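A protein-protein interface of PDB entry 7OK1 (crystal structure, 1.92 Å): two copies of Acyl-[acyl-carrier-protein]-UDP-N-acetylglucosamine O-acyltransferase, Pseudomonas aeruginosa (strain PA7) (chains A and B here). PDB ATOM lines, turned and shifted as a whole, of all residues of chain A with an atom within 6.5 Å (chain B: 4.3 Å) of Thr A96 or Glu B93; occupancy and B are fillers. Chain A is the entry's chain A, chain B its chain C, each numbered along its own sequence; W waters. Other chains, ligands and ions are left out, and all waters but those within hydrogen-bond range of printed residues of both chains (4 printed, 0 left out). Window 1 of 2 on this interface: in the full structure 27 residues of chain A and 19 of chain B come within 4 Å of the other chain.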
ATOM      1  N   PHE A  64     -12.895  -8.036   4.861  1.00  0.00           N
ATOM      2  CA  PHE A  64     -12.014  -8.176   6.040  1.00  0.00           C
ATOM      3  C   PHE A  64     -11.299  -6.891   6.440  1.00  0.00           C
ATOM      4  O   PHE A  64     -10.489  -6.910   7.370  1.00  0.00           O
ATOM      5  CB  PHE A  64     -11.009  -9.371   5.890  1.00  0.00           C
ATOM      6  CG  PHE A  64     -11.645 -10.612   5.300  1.00  0.00           C
ATOM      7  CD1 PHE A  64     -12.759 -11.198   5.903  1.00  0.00           C
ATOM      8  CD2 PHE A  64     -11.158 -11.169   4.125  1.00  0.00           C
ATOM      9  CE1 PHE A  64     -13.379 -12.314   5.325  1.00  0.00           C
ATOM     10  CE2 PHE A  64     -11.761 -12.305   3.560  1.00  0.00           C
ATOM     11  CZ  PHE A  64     -12.872 -12.862   4.154  1.00  0.00           C
ATOM     12  N   SER A  65     -11.680  -5.760   5.825  1.00  0.00           N
ATOM     13  CA  SER A  65     -11.210  -4.425   6.185  1.00  0.00           C
ATOM     14  C   SER A  65     -11.963  -3.949   7.424  1.00  0.00           C
ATOM     15  O   SER A  65     -13.137  -4.267   7.580  1.00  0.00           O
ATOM     16  CB  SER A  65     -11.467  -3.438   5.043  1.00  0.00           C
ATOM     17  OG  SER A  65     -10.770  -3.852   3.883  1.00  0.00           O
ATOM     18  N   SER A  66     -11.290  -3.195   8.296  1.00  0.00           N
ATOM     19  CA  SER A  66     -11.858  -2.560   9.491  1.00  0.00           C
ATOM     20  C   SER A  66     -11.516  -1.098   9.364  1.00  0.00           C
ATOM     21  O   SER A  66     -10.377  -0.710   9.599  1.00  0.00           O
ATOM     22  CB  SER A  66     -11.288  -3.152  10.779  1.00  0.00           C
ATOM     23  OG  SER A  66     -11.849  -4.438  10.966  1.00  0.00           O
ATOM     24  N   VAL A  67     -12.478  -0.309   8.888  1.00  0.00           N
ATOM     25  CA  VAL A  67     -12.284   1.095   8.573  1.00  0.00           C
ATOM     26  C   VAL A  67     -13.100   1.979   9.509  1.00  0.00           C
ATOM     27  O   VAL A  67     -14.326   1.900   9.520  1.00  0.00           O
ATOM     28  CB  VAL A  67     -12.630   1.360   7.064  1.00  0.00           C
ATOM     29  CG1 VAL A  67     -12.593   2.851   6.714  1.00  0.00           C
ATOM     30  CG2 VAL A  67     -11.742   0.564   6.118  1.00  0.00           C
ATOM     31  N   GLY A  68     -12.411   2.846  10.239  1.00  0.00           N
ATOM     32  CA  GLY A  68     -13.035   3.788  11.155  1.00  0.00           C
ATOM     33  C   GLY A  68     -13.026   3.358  12.604  1.00  0.00           C
ATOM     34  O   GLY A  68     -13.731   3.954  13.413  1.00  0.00           O
ATOM     35  N   GLU A  69     -12.208   2.345  12.960  1.00  0.00           N
ATOM     36  CA  GLU A  69     -12.093   1.898  14.362  1.00  0.00           C
ATOM     37  C   GLU A  69     -11.350   2.956  15.204  1.00  0.00           C
ATOM     38  O   GLU A  69     -10.668   3.833  14.673  1.00  0.00           O
ATOM     39  CB  GLU A  69     -11.275   0.587  14.442  1.00  0.00           C
ATOM     40  CG  GLU A  69     -12.010  -0.684  14.039  1.00  0.00           C
ATOM     41  CD  GLU A  69     -13.067  -1.190  15.001  1.00  0.00           C
ATOM     42  OE1 GLU A  69     -13.072  -0.769  16.177  1.00  0.00           O
ATOM     43  OE2 GLU A  69     -13.903  -2.011  14.567  1.00  0.00           O
ATOM     44  N   ASP A  70     -11.445   2.822  16.512  1.00  0.00           N
ATOM     45  CA  ASP A  70     -10.696   3.601  17.474  1.00  0.00           C
ATOM     46  C   ASP A  70      -9.274   3.045  17.426  1.00  0.00           C
ATOM     47  O   ASP A  70      -9.078   1.829  17.251  1.00  0.00           O
ATOM     48  CB  ASP A  70     -11.184   3.279  18.909  1.00  0.00           C
ATOM     49  CG  ASP A  70     -12.615   3.617  19.269  1.00  0.00           C
ATOM     50  OD1 ASP A  70     -13.307   4.261  18.437  1.00  0.00           O
ATOM     51  OD2 ASP A  70     -13.041   3.254  20.391  1.00  0.00           O
ATOM     52  N   PRO A  72      -6.136   1.547  19.247  1.00  0.00           N
ATOM     53  CA  PRO A  72      -5.978   0.873  20.541  1.00  0.00           C
ATOM     54  C   PRO A  72      -5.036   1.628  21.484  1.00  0.00           C
ATOM     55  O   PRO A  72      -5.025   1.320  22.673  1.00  0.00           O
ATOM     56  CB  PRO A  72      -5.374  -0.482  20.158  1.00  0.00           C
ATOM     57  CG  PRO A  72      -4.600  -0.213  18.917  1.00  0.00           C
ATOM     58  CD  PRO A  72      -5.349   0.871  18.185  1.00  0.00           C
ATOM     59  N   ILE A  91      -9.599   0.402  -1.269  1.00  0.00           N
ATOM     60  CA  ILE A  91      -9.117  -0.119   0.001  1.00  0.00           C
ATOM     61  C   ILE A  91      -9.245  -1.633  -0.138  1.00  0.00           C
ATOM     62  O   ILE A  91     -10.348  -2.176  -0.223  1.00  0.00           O
ATOM     63  CB  ILE A  91      -9.867   0.504   1.208  1.00  0.00           C
ATOM     64  CG1 ILE A  91      -9.613   2.025   1.314  1.00  0.00           C
ATOM     65  CG2 ILE A  91      -9.540  -0.226   2.521  1.00  0.00           C
ATOM     66  CD1 ILE A  91     -10.639   2.806   2.213  1.00  0.00           C
ATOM     67  N   GLY A  94      -8.451  -6.622   4.199  1.00  0.00           N
ATOM     68  CA  GLY A  94      -7.803  -6.595   5.506  1.00  0.00           C
ATOM     69  C   GLY A  94      -7.170  -5.317   6.004  1.00  0.00           C
ATOM     70  O   GLY A  94      -6.503  -5.338   7.040  1.00  0.00           O
ATOM     71  N   VAL A  95      -7.361  -4.206   5.296  1.00  0.00           N
ATOM     72  CA  VAL A  95      -6.840  -2.879   5.665  1.00  0.00           C
ATOM     73  C   VAL A  95      -7.483  -2.375   6.977  1.00  0.00           C
ATOM     74  O   VAL A  95      -8.690  -2.560   7.189  1.00  0.00           O
ATOM     75  CB  VAL A  95      -7.013  -1.872   4.490  1.00  0.00           C
ATOM     76  CG1 VAL A  95      -6.661  -0.426   4.900  1.00  0.00           C
ATOM     77  CG2 VAL A  95      -6.198  -2.315   3.268  1.00  0.00           C
ATOM     78  N   THR A  96      -6.666  -1.772   7.859  1.00  0.00           N
ATOM     79  CA  THR A  96      -7.145  -1.174   9.110  1.00  0.00           C
ATOM     80  C   THR A  96      -6.877   0.343   9.036  1.00  0.00           C
ATOM     81  O   THR A  96      -5.766   0.762   8.698  1.00  0.00           O
ATOM     82  CB  THR A  96      -6.529  -1.829  10.347  1.00  0.00           C
ATOM     83  OG1 THR A  96      -5.112  -1.692  10.285  1.00  0.00           O
ATOM     84  CG2 THR A  96      -6.914  -3.316  10.496  1.00  0.00           C
ATOM     85  N   ILE A  97      -7.921   1.152   9.250  1.00  0.00           N
ATOM     86  CA  ILE A  97      -7.831   2.610   9.235  1.00  0.00           C
ATOM     87  C   ILE A  97      -8.471   3.115  10.520  1.00  0.00           C
ATOM     88  O   ILE A  97      -9.638   2.820  10.790  1.00  0.00           O
ATOM     89  CB  ILE A  97      -8.454   3.261   7.965  1.00  0.00           C
ATOM     90  CG1 ILE A  97      -8.017   2.526   6.662  1.00  0.00           C
ATOM     91  CG2 ILE A  97      -8.145   4.776   7.918  1.00  0.00           C
ATOM     92  CD1 ILE A  97      -8.568   3.116   5.306  1.00  0.00           C
ATOM     93  N   HIS A  98      -7.706   3.854  11.318  1.00  0.00           N
ATOM     94  CA  HIS A  98      -8.184   4.370  12.600  1.00  0.00           C
ATOM     95  C   HIS A  98      -8.531   5.826  12.528  1.00  0.00           C
ATOM     96  O   HIS A  98      -7.975   6.542  11.697  1.00  0.00           O
ATOM     97  CB  HIS A  98      -7.177   4.095  13.727  1.00  0.00           C
ATOM     98  CG  HIS A  98      -6.956   2.639  13.968  1.00  0.00           C
ATOM     99  ND1 HIS A  98      -5.908   2.190  14.745  1.00  0.00           N
ATOM    100  CD2 HIS A  98      -7.645   1.566  13.501  1.00  0.00           C
ATOM    101  CE1 HIS A  98      -5.992   0.867  14.725  1.00  0.00           C
ATOM    102  NE2 HIS A  98      -7.010   0.450  13.971  1.00  0.00           N
ATOM    103  N   TYR A 119      -3.953  -5.434   3.819  1.00  0.00           N
ATOM    104  CA  TYR A 119      -3.392  -5.429   5.186  1.00  0.00           C
ATOM    105  C   TYR A 119      -2.556  -4.209   5.513  1.00  0.00           C
ATOM    106  O   TYR A 119      -1.865  -4.204   6.538  1.00  0.00           O
ATOM    107  CB  TYR A 119      -2.616  -6.740   5.499  1.00  0.00           C
ATOM    108  CG  TYR A 119      -3.515  -7.942   5.323  1.00  0.00           C
ATOM    109  CD1 TYR A 119      -4.523  -8.220   6.243  1.00  0.00           C
ATOM    110  CD2 TYR A 119      -3.472  -8.703   4.154  1.00  0.00           C
ATOM    111  CE1 TYR A 119      -5.437  -9.244   6.029  1.00  0.00           C
ATOM    112  CE2 TYR A 119      -4.382  -9.738   3.932  1.00  0.00           C
ATOM    113  CZ  TYR A 119      -5.362 -10.004   4.875  1.00  0.00           C
ATOM    114  OH  TYR A 119      -6.297 -10.985   4.668  1.00  0.00           O
ATOM    115  N   ALA A 120      -2.677  -3.138   4.702  1.00  0.00           N
ATOM    116  CA  ALA A 120      -2.013  -1.857   5.007  1.00  0.00           C
ATOM    117  C   ALA A 120      -2.690  -1.273   6.270  1.00  0.00           C
ATOM    118  O   ALA A 120      -3.850  -1.597   6.578  1.00  0.00           O
ATOM    119  CB  ALA A 120      -2.133  -0.873   3.833  1.00  0.00           C
ATOM    120  N   HIS A 121      -1.933  -0.493   7.036  1.00  0.00           N
ATOM    121  CA  HIS A 121      -2.416   0.110   8.263  1.00  0.00           C
ATOM    122  C   HIS A 121      -2.230   1.592   8.239  1.00  0.00           C
ATOM    123  O   HIS A 121      -1.108   2.076   8.031  1.00  0.00           O
ATOM    124  CB  HIS A 121      -1.725  -0.486   9.493  1.00  0.00           C
ATOM    125  CG  HIS A 121      -2.038   0.256  10.757  1.00  0.00           C
ATOM    126  ND1 HIS A 121      -3.229   0.047  11.440  1.00  0.00           N
ATOM    127  CD2 HIS A 121      -1.331   1.224  11.389  1.00  0.00           C
ATOM    128  CE1 HIS A 121      -3.186   0.850  12.491  1.00  0.00           C
ATOM    129  NE2 HIS A 121      -2.070   1.590  12.498  1.00  0.00           N
ATOM    130  N   ILE A 122      -3.337   2.323   8.494  1.00  0.00           N
ATOM    131  CA  ILE A 122      -3.330   3.768   8.573  1.00  0.00           C
ATOM    132  C   ILE A 122      -3.679   4.176  10.006  1.00  0.00           C
ATOM    133  O   ILE A 122      -4.843   4.132  10.430  1.00  0.00           O
ATOM    134  CB  ILE A 122      -4.213   4.400   7.465  1.00  0.00           C
ATOM    135  CG1 ILE A 122      -3.702   3.940   6.056  1.00  0.00           C
ATOM    136  CG2 ILE A 122      -4.228   5.953   7.596  1.00  0.00           C
ATOM    137  CD1 ILE A 122      -4.647   4.142   4.904  1.00  0.00           C
ATOM    138  N   GLY A 123      -2.650   4.506  10.770  1.00  0.00           N
ATOM    139  CA  GLY A 123      -2.822   4.891  12.172  1.00  0.00           C
ATOM    140  C   GLY A 123      -3.490   6.234  12.385  1.00  0.00           C
ATOM    141  O   GLY A 123      -3.557   7.046  11.461  1.00  0.00           O
ATOM    142  N   TYR B  62     -11.448  -8.627  18.847  1.00  0.00           N
ATOM    143  CA  TYR B  62     -11.914  -7.968  17.637  1.00  0.00           C
ATOM    144  C   TYR B  62     -12.053  -8.924  16.468  1.00  0.00           C
ATOM    145  O   TYR B  62     -11.459  -9.990  16.460  1.00  0.00           O
ATOM    146  CB  TYR B  62     -10.971  -6.799  17.284  1.00  0.00           C
ATOM    147  CG  TYR B  62     -11.217  -5.535  18.084  1.00  0.00           C
ATOM    148  CD1 TYR B  62     -10.905  -5.467  19.443  1.00  0.00           C
ATOM    149  CD2 TYR B  62     -11.753  -4.397  17.483  1.00  0.00           C
ATOM    150  CE1 TYR B  62     -11.105  -4.290  20.175  1.00  0.00           C
ATOM    151  CE2 TYR B  62     -11.998  -3.232  18.218  1.00  0.00           C
ATOM    152  CZ  TYR B  62     -11.669  -3.184  19.561  1.00  0.00           C
ATOM    153  OH  TYR B  62     -11.857  -2.010  20.257  1.00  0.00           O
ATOM    154  N   GLN B  63     -12.846  -8.507  15.479  1.00  0.00           N
ATOM    155  CA  GLN B  63     -13.127  -9.192  14.219  1.00  0.00           C
ATOM    156  C   GLN B  63     -11.897  -9.717  13.484  1.00  0.00           C
ATOM    157  O   GLN B  63     -10.837  -9.073  13.468  1.00  0.00           O
ATOM    158  CB  GLN B  63     -13.915  -8.269  13.249  1.00  0.00           C
ATOM    159  CG  GLN B  63     -13.254  -6.901  12.934  1.00  0.00           C
ATOM    160  CD  GLN B  63     -13.648  -5.784  13.878  1.00  0.00           C
ATOM    161  OE1 GLN B  63     -14.233  -5.995  14.927  1.00  0.00           O
ATOM    162  NE2 GLN B  63     -13.323  -4.566  13.529  1.00  0.00           N
ATOM    163  N   SER B  65     -10.057 -12.232  13.949  1.00  0.00           N
ATOM    164  CA  SER B  65      -9.096 -12.934  14.807  1.00  0.00           C
ATOM    165  C   SER B  65      -9.386 -14.443  14.776  1.00  0.00           C
ATOM    166  O   SER B  65     -10.551 -14.847  14.682  1.00  0.00           O
ATOM    167  CB  SER B  65      -9.200 -12.459  16.255  1.00  0.00           C
ATOM    168  OG  SER B  65      -8.641 -11.163  16.403  1.00  0.00           O
ATOM    169  N   ARG B  92      -6.728  -7.357  19.099  1.00  0.00           N
ATOM    170  CA  ARG B  92      -7.254  -6.570  17.983  1.00  0.00           C
ATOM    171  C   ARG B  92      -7.529  -7.428  16.758  1.00  0.00           C
ATOM    172  O   ARG B  92      -7.454  -8.646  16.835  1.00  0.00           O
ATOM    173  CB  ARG B  92      -6.349  -5.346  17.678  1.00  0.00           C
ATOM    174  CG  ARG B  92      -6.302  -4.286  18.822  1.00  0.00           C
ATOM    175  CD  ARG B  92      -7.602  -3.491  19.024  1.00  0.00           C
ATOM    176  NE  ARG B  92      -8.037  -2.828  17.795  1.00  0.00           N
ATOM    177  CZ  ARG B  92      -8.509  -1.584  17.714  1.00  0.00           C
ATOM    178  NH1 ARG B  92      -8.655  -0.844  18.810  1.00  0.00           N
ATOM    179  NH2 ARG B  92      -8.850  -1.076  16.538  1.00  0.00           N
ATOM    180  N   GLU B  93      -7.937  -6.804  15.662  1.00  0.00           N
ATOM    181  CA  GLU B  93      -8.282  -7.483  14.410  1.00  0.00           C
ATOM    182  C   GLU B  93      -7.180  -8.337  13.756  1.00  0.00           C
ATOM    183  O   GLU B  93      -6.016  -7.934  13.671  1.00  0.00           O
ATOM    184  CB  GLU B  93      -8.834  -6.487  13.368  1.00  0.00           C
ATOM    185  CG  GLU B  93      -8.092  -5.183  13.310  1.00  0.00           C
ATOM    186  CD  GLU B  93      -8.682  -4.072  14.151  1.00  0.00           C
ATOM    187  OE1 GLU B  93      -9.861  -3.716  13.935  1.00  0.00           O
ATOM    188  OE2 GLU B  93      -7.944  -3.526  14.998  1.00  0.00           O
ATOM    189  N   GLY B  94      -7.604  -9.495  13.263  1.00  0.00           N
ATOM    190  CA  GLY B  94      -6.792 -10.457  12.537  1.00  0.00           C
ATOM    191  C   GLY B  94      -5.663 -11.134  13.294  1.00  0.00           C
ATOM    192  O   GLY B  94      -4.783 -11.719  12.675  1.00  0.00           O
ATOM    193  N   VAL B  95      -5.663 -11.041  14.627  1.00  0.00           N
ATOM    194  CA  VAL B  95      -4.648 -11.670  15.474  1.00  0.00           C
ATOM    195  C   VAL B  95      -4.787 -13.209  15.404  1.00  0.00           C
ATOM    196  O   VAL B  95      -5.898 -13.733  15.481  1.00  0.00           O
ATOM    197  CB  VAL B  95      -4.768 -11.137  16.936  1.00  0.00           C
ATOM    198  CG1 VAL B  95      -3.998 -12.009  17.927  1.00  0.00           C
ATOM    199  CG2 VAL B  95      -4.322  -9.672  17.028  1.00  0.00           C
ATOM    200  N   ALA B 118      -3.375  -5.436  15.889  1.00  0.00           N
ATOM    201  CA  ALA B 118      -3.764  -6.004  14.606  1.00  0.00           C
ATOM    202  C   ALA B 118      -2.714  -6.879  13.927  1.00  0.00           C
ATOM    203  O   ALA B 118      -1.558  -6.481  13.790  1.00  0.00           O
ATOM    204  CB  ALA B 118      -4.232  -4.912  13.659  1.00  0.00           C
ATOM    205  N   TYR B 119      -3.135  -8.102  13.545  1.00  0.00           N
ATOM    206  CA  TYR B 119      -2.347  -9.099  12.788  1.00  0.00           C
ATOM    207  C   TYR B 119      -1.131  -9.615  13.534  1.00  0.00           C
ATOM    208  O   TYR B 119      -0.297 -10.255  12.929  1.00  0.00           O
ATOM    209  CB  TYR B 119      -1.979  -8.582  11.374  1.00  0.00           C
ATOM    210  CG  TYR B 119      -3.224  -8.209  10.628  1.00  0.00           C
ATOM    211  CD1 TYR B 119      -4.198  -9.161  10.345  1.00  0.00           C
ATOM    212  CD2 TYR B 119      -3.514  -6.875  10.341  1.00  0.00           C
ATOM    213  CE1 TYR B 119      -5.401  -8.811   9.742  1.00  0.00           C
ATOM    214  CE2 TYR B 119      -4.732  -6.506   9.765  1.00  0.00           C
ATOM    215  CZ  TYR B 119      -5.680  -7.478   9.490  1.00  0.00           C
ATOM    216  OH  TYR B 119      -6.861  -7.142   8.899  1.00  0.00           O
HETATM  217  O   HOH W   1      -9.313  -0.774  12.243  1.00  0.00           O
HETATM  218  O   HOH W   2     -12.843   0.374  18.434  1.00  0.00           O
HETATM  219  O   HOH W   3      -9.539  -5.668   9.603  1.00  0.00           O
HETATM  220  O   HOH W   4      -8.792  -8.861   8.521  1.00  0.00           O
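The side-chain amide nitrogen (NE2) of Gln B63 is in hydrogen-bond range of the side-chain hydroxyl (OG) of Ser A66.
OE2 of Glu A69 lies within hydrogen-bond range of NE2 of Gln B63 (2.8 Å).
O of Asp A70 sits at hydrogen-bond distance from NH2 of Arg B92.
O of Gly A94 lies within hydrogen-bond range of OH of Tyr B119.
The backbone NH of Glu A69 lies within hydrogen-bond range of the backbone carbonyl oxygen of Ile A97, at 3.4 Å.
N of Ile A122 is in hydrogen-bond range of O of Thr A96 (2.9 Å).
N of His A98 is in hydrogen-bond range of O of Ile A122 (3.0 Å).
The side-chain hydroxyl (OG) of Ser B65 is in hydrogen-bond range of the backbone carbonyl oxygen (O) of Arg B92, 2.8 Å away.
OE2 of Glu B93 lies within salt-bridge range of NE of Arg B92 (2.9 Å).
The backbone NH (N) of Tyr B119 lies within hydrogen-bond range of the backbone carbonyl oxygen (O) of Glu B93 (2.9 Å).
Tyr B119 touches Phe A64.
Ser A66 touches Glu B93.
Glu A69 touches Tyr B62 (OE1 to CE2, 3.4 Å).
Glu A69 touches Arg B92.
OE1 of Glu B93 touches CG of Glu A69 (3.7 Å).
Pro A72 touches Arg B92 (N to NH1, 3.5 Å).
CG of Glu B93 touches CG2 of Thr A96, at 3.6 Å.
CG2 of Thr A96 touches CE2 of Tyr B119, 3.9 Å away.
NE2 of His A98 touches NH2 of Arg B92, at 3.5 Å.
Tyr B119 touches Tyr A119.
Of the printed residues of chain B, Glu A69 touches Tyr B62, Gln B63, Arg B92 and Glu B93.
Of the printed residues of chain B, Pro A72 touches Arg B92 (3.5 Å).
Of chain B, only Glu B93 and Tyr B119 come within 4 Å of Thr A96.
Printed residues of chain B within 4 Å of His A98: Arg B92.
Of the printed residues of chain A, Tyr B62 touches Glu A69 (3.4 Å).
Ser B65 touches none of the printed residues of chain A.
Glu B93 touches three residues of chain A.
Of the 9 printed residues of chain B, 5 touch a printed residue of chain A.
Printed residues of chain B that touch a printed residue of chain A: Tyr B62, Gln B63, Arg B92, Glu B93 and Tyr B119.
Hydrophobic or aromatic side chains of chain B that line the printed part of chain A: Tyr B62 and Tyr B119.
Of the 19 printed residues of chain A, 9 touch a printed residue of chain B.
Printed residues of chain A that touch a printed residue of chain B: Phe A64, Ser A66, Glu A69, Asp A70, Pro A72, Gly A94, Thr A96, His A98 and Tyr A119.
Hydrophobic or aromatic side chains of chain A that line the printed part of chain B: Pro A72, His A98 and Tyr A119.
Among the printed residues, 14 pairs touch across the chains.
Among the printed residues, no Asp or Glu carboxylate lies within 4 Å of a Lys or Arg side-chain nitrogen of the other chain.
Gly A94 touches Tyr B119, but with the chains exchanged Tyr A119 does not touch Gly B94 (6.8 Å).
Tyr A119 touches its own counterpart, Tyr B119.
Positions printed for both chains: 65, 94, 95 and 119.
Of the 14 pairs that touch across the chains among the printed residues, 1 has its exchanged pair printed and touching as well.
Water W2 lies within hydrogen-bond range of the side-chain carboxylate (OE1) of Glu A69 (2.5 Å), the side-chain hydroxyl (OH) of Tyr B62 (3.2 Å) and the backbone NH (N) of Asp A70 (3.4 Å).
Water W4 lies within hydrogen-bond range of the side-chain hydroxyl (OH) of Tyr B119 and the backbone carbonyl oxygen (O) of Phe A64.
Water W3 lies within hydrogen-bond range of the backbone carbonyl oxygen of Phe A64 (2.7 Å), the side-chain hydroxyl of Ser A66 (3.0 Å) and the side-chain hydroxyl of Tyr B119 (3.1 Å).
Water W1 lies within hydrogen-bond range of the backbone carbonyl oxygen of Ser A66, a ring nitrogen (NE2) of His A98 and the side-chain carboxylate of Glu B93.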
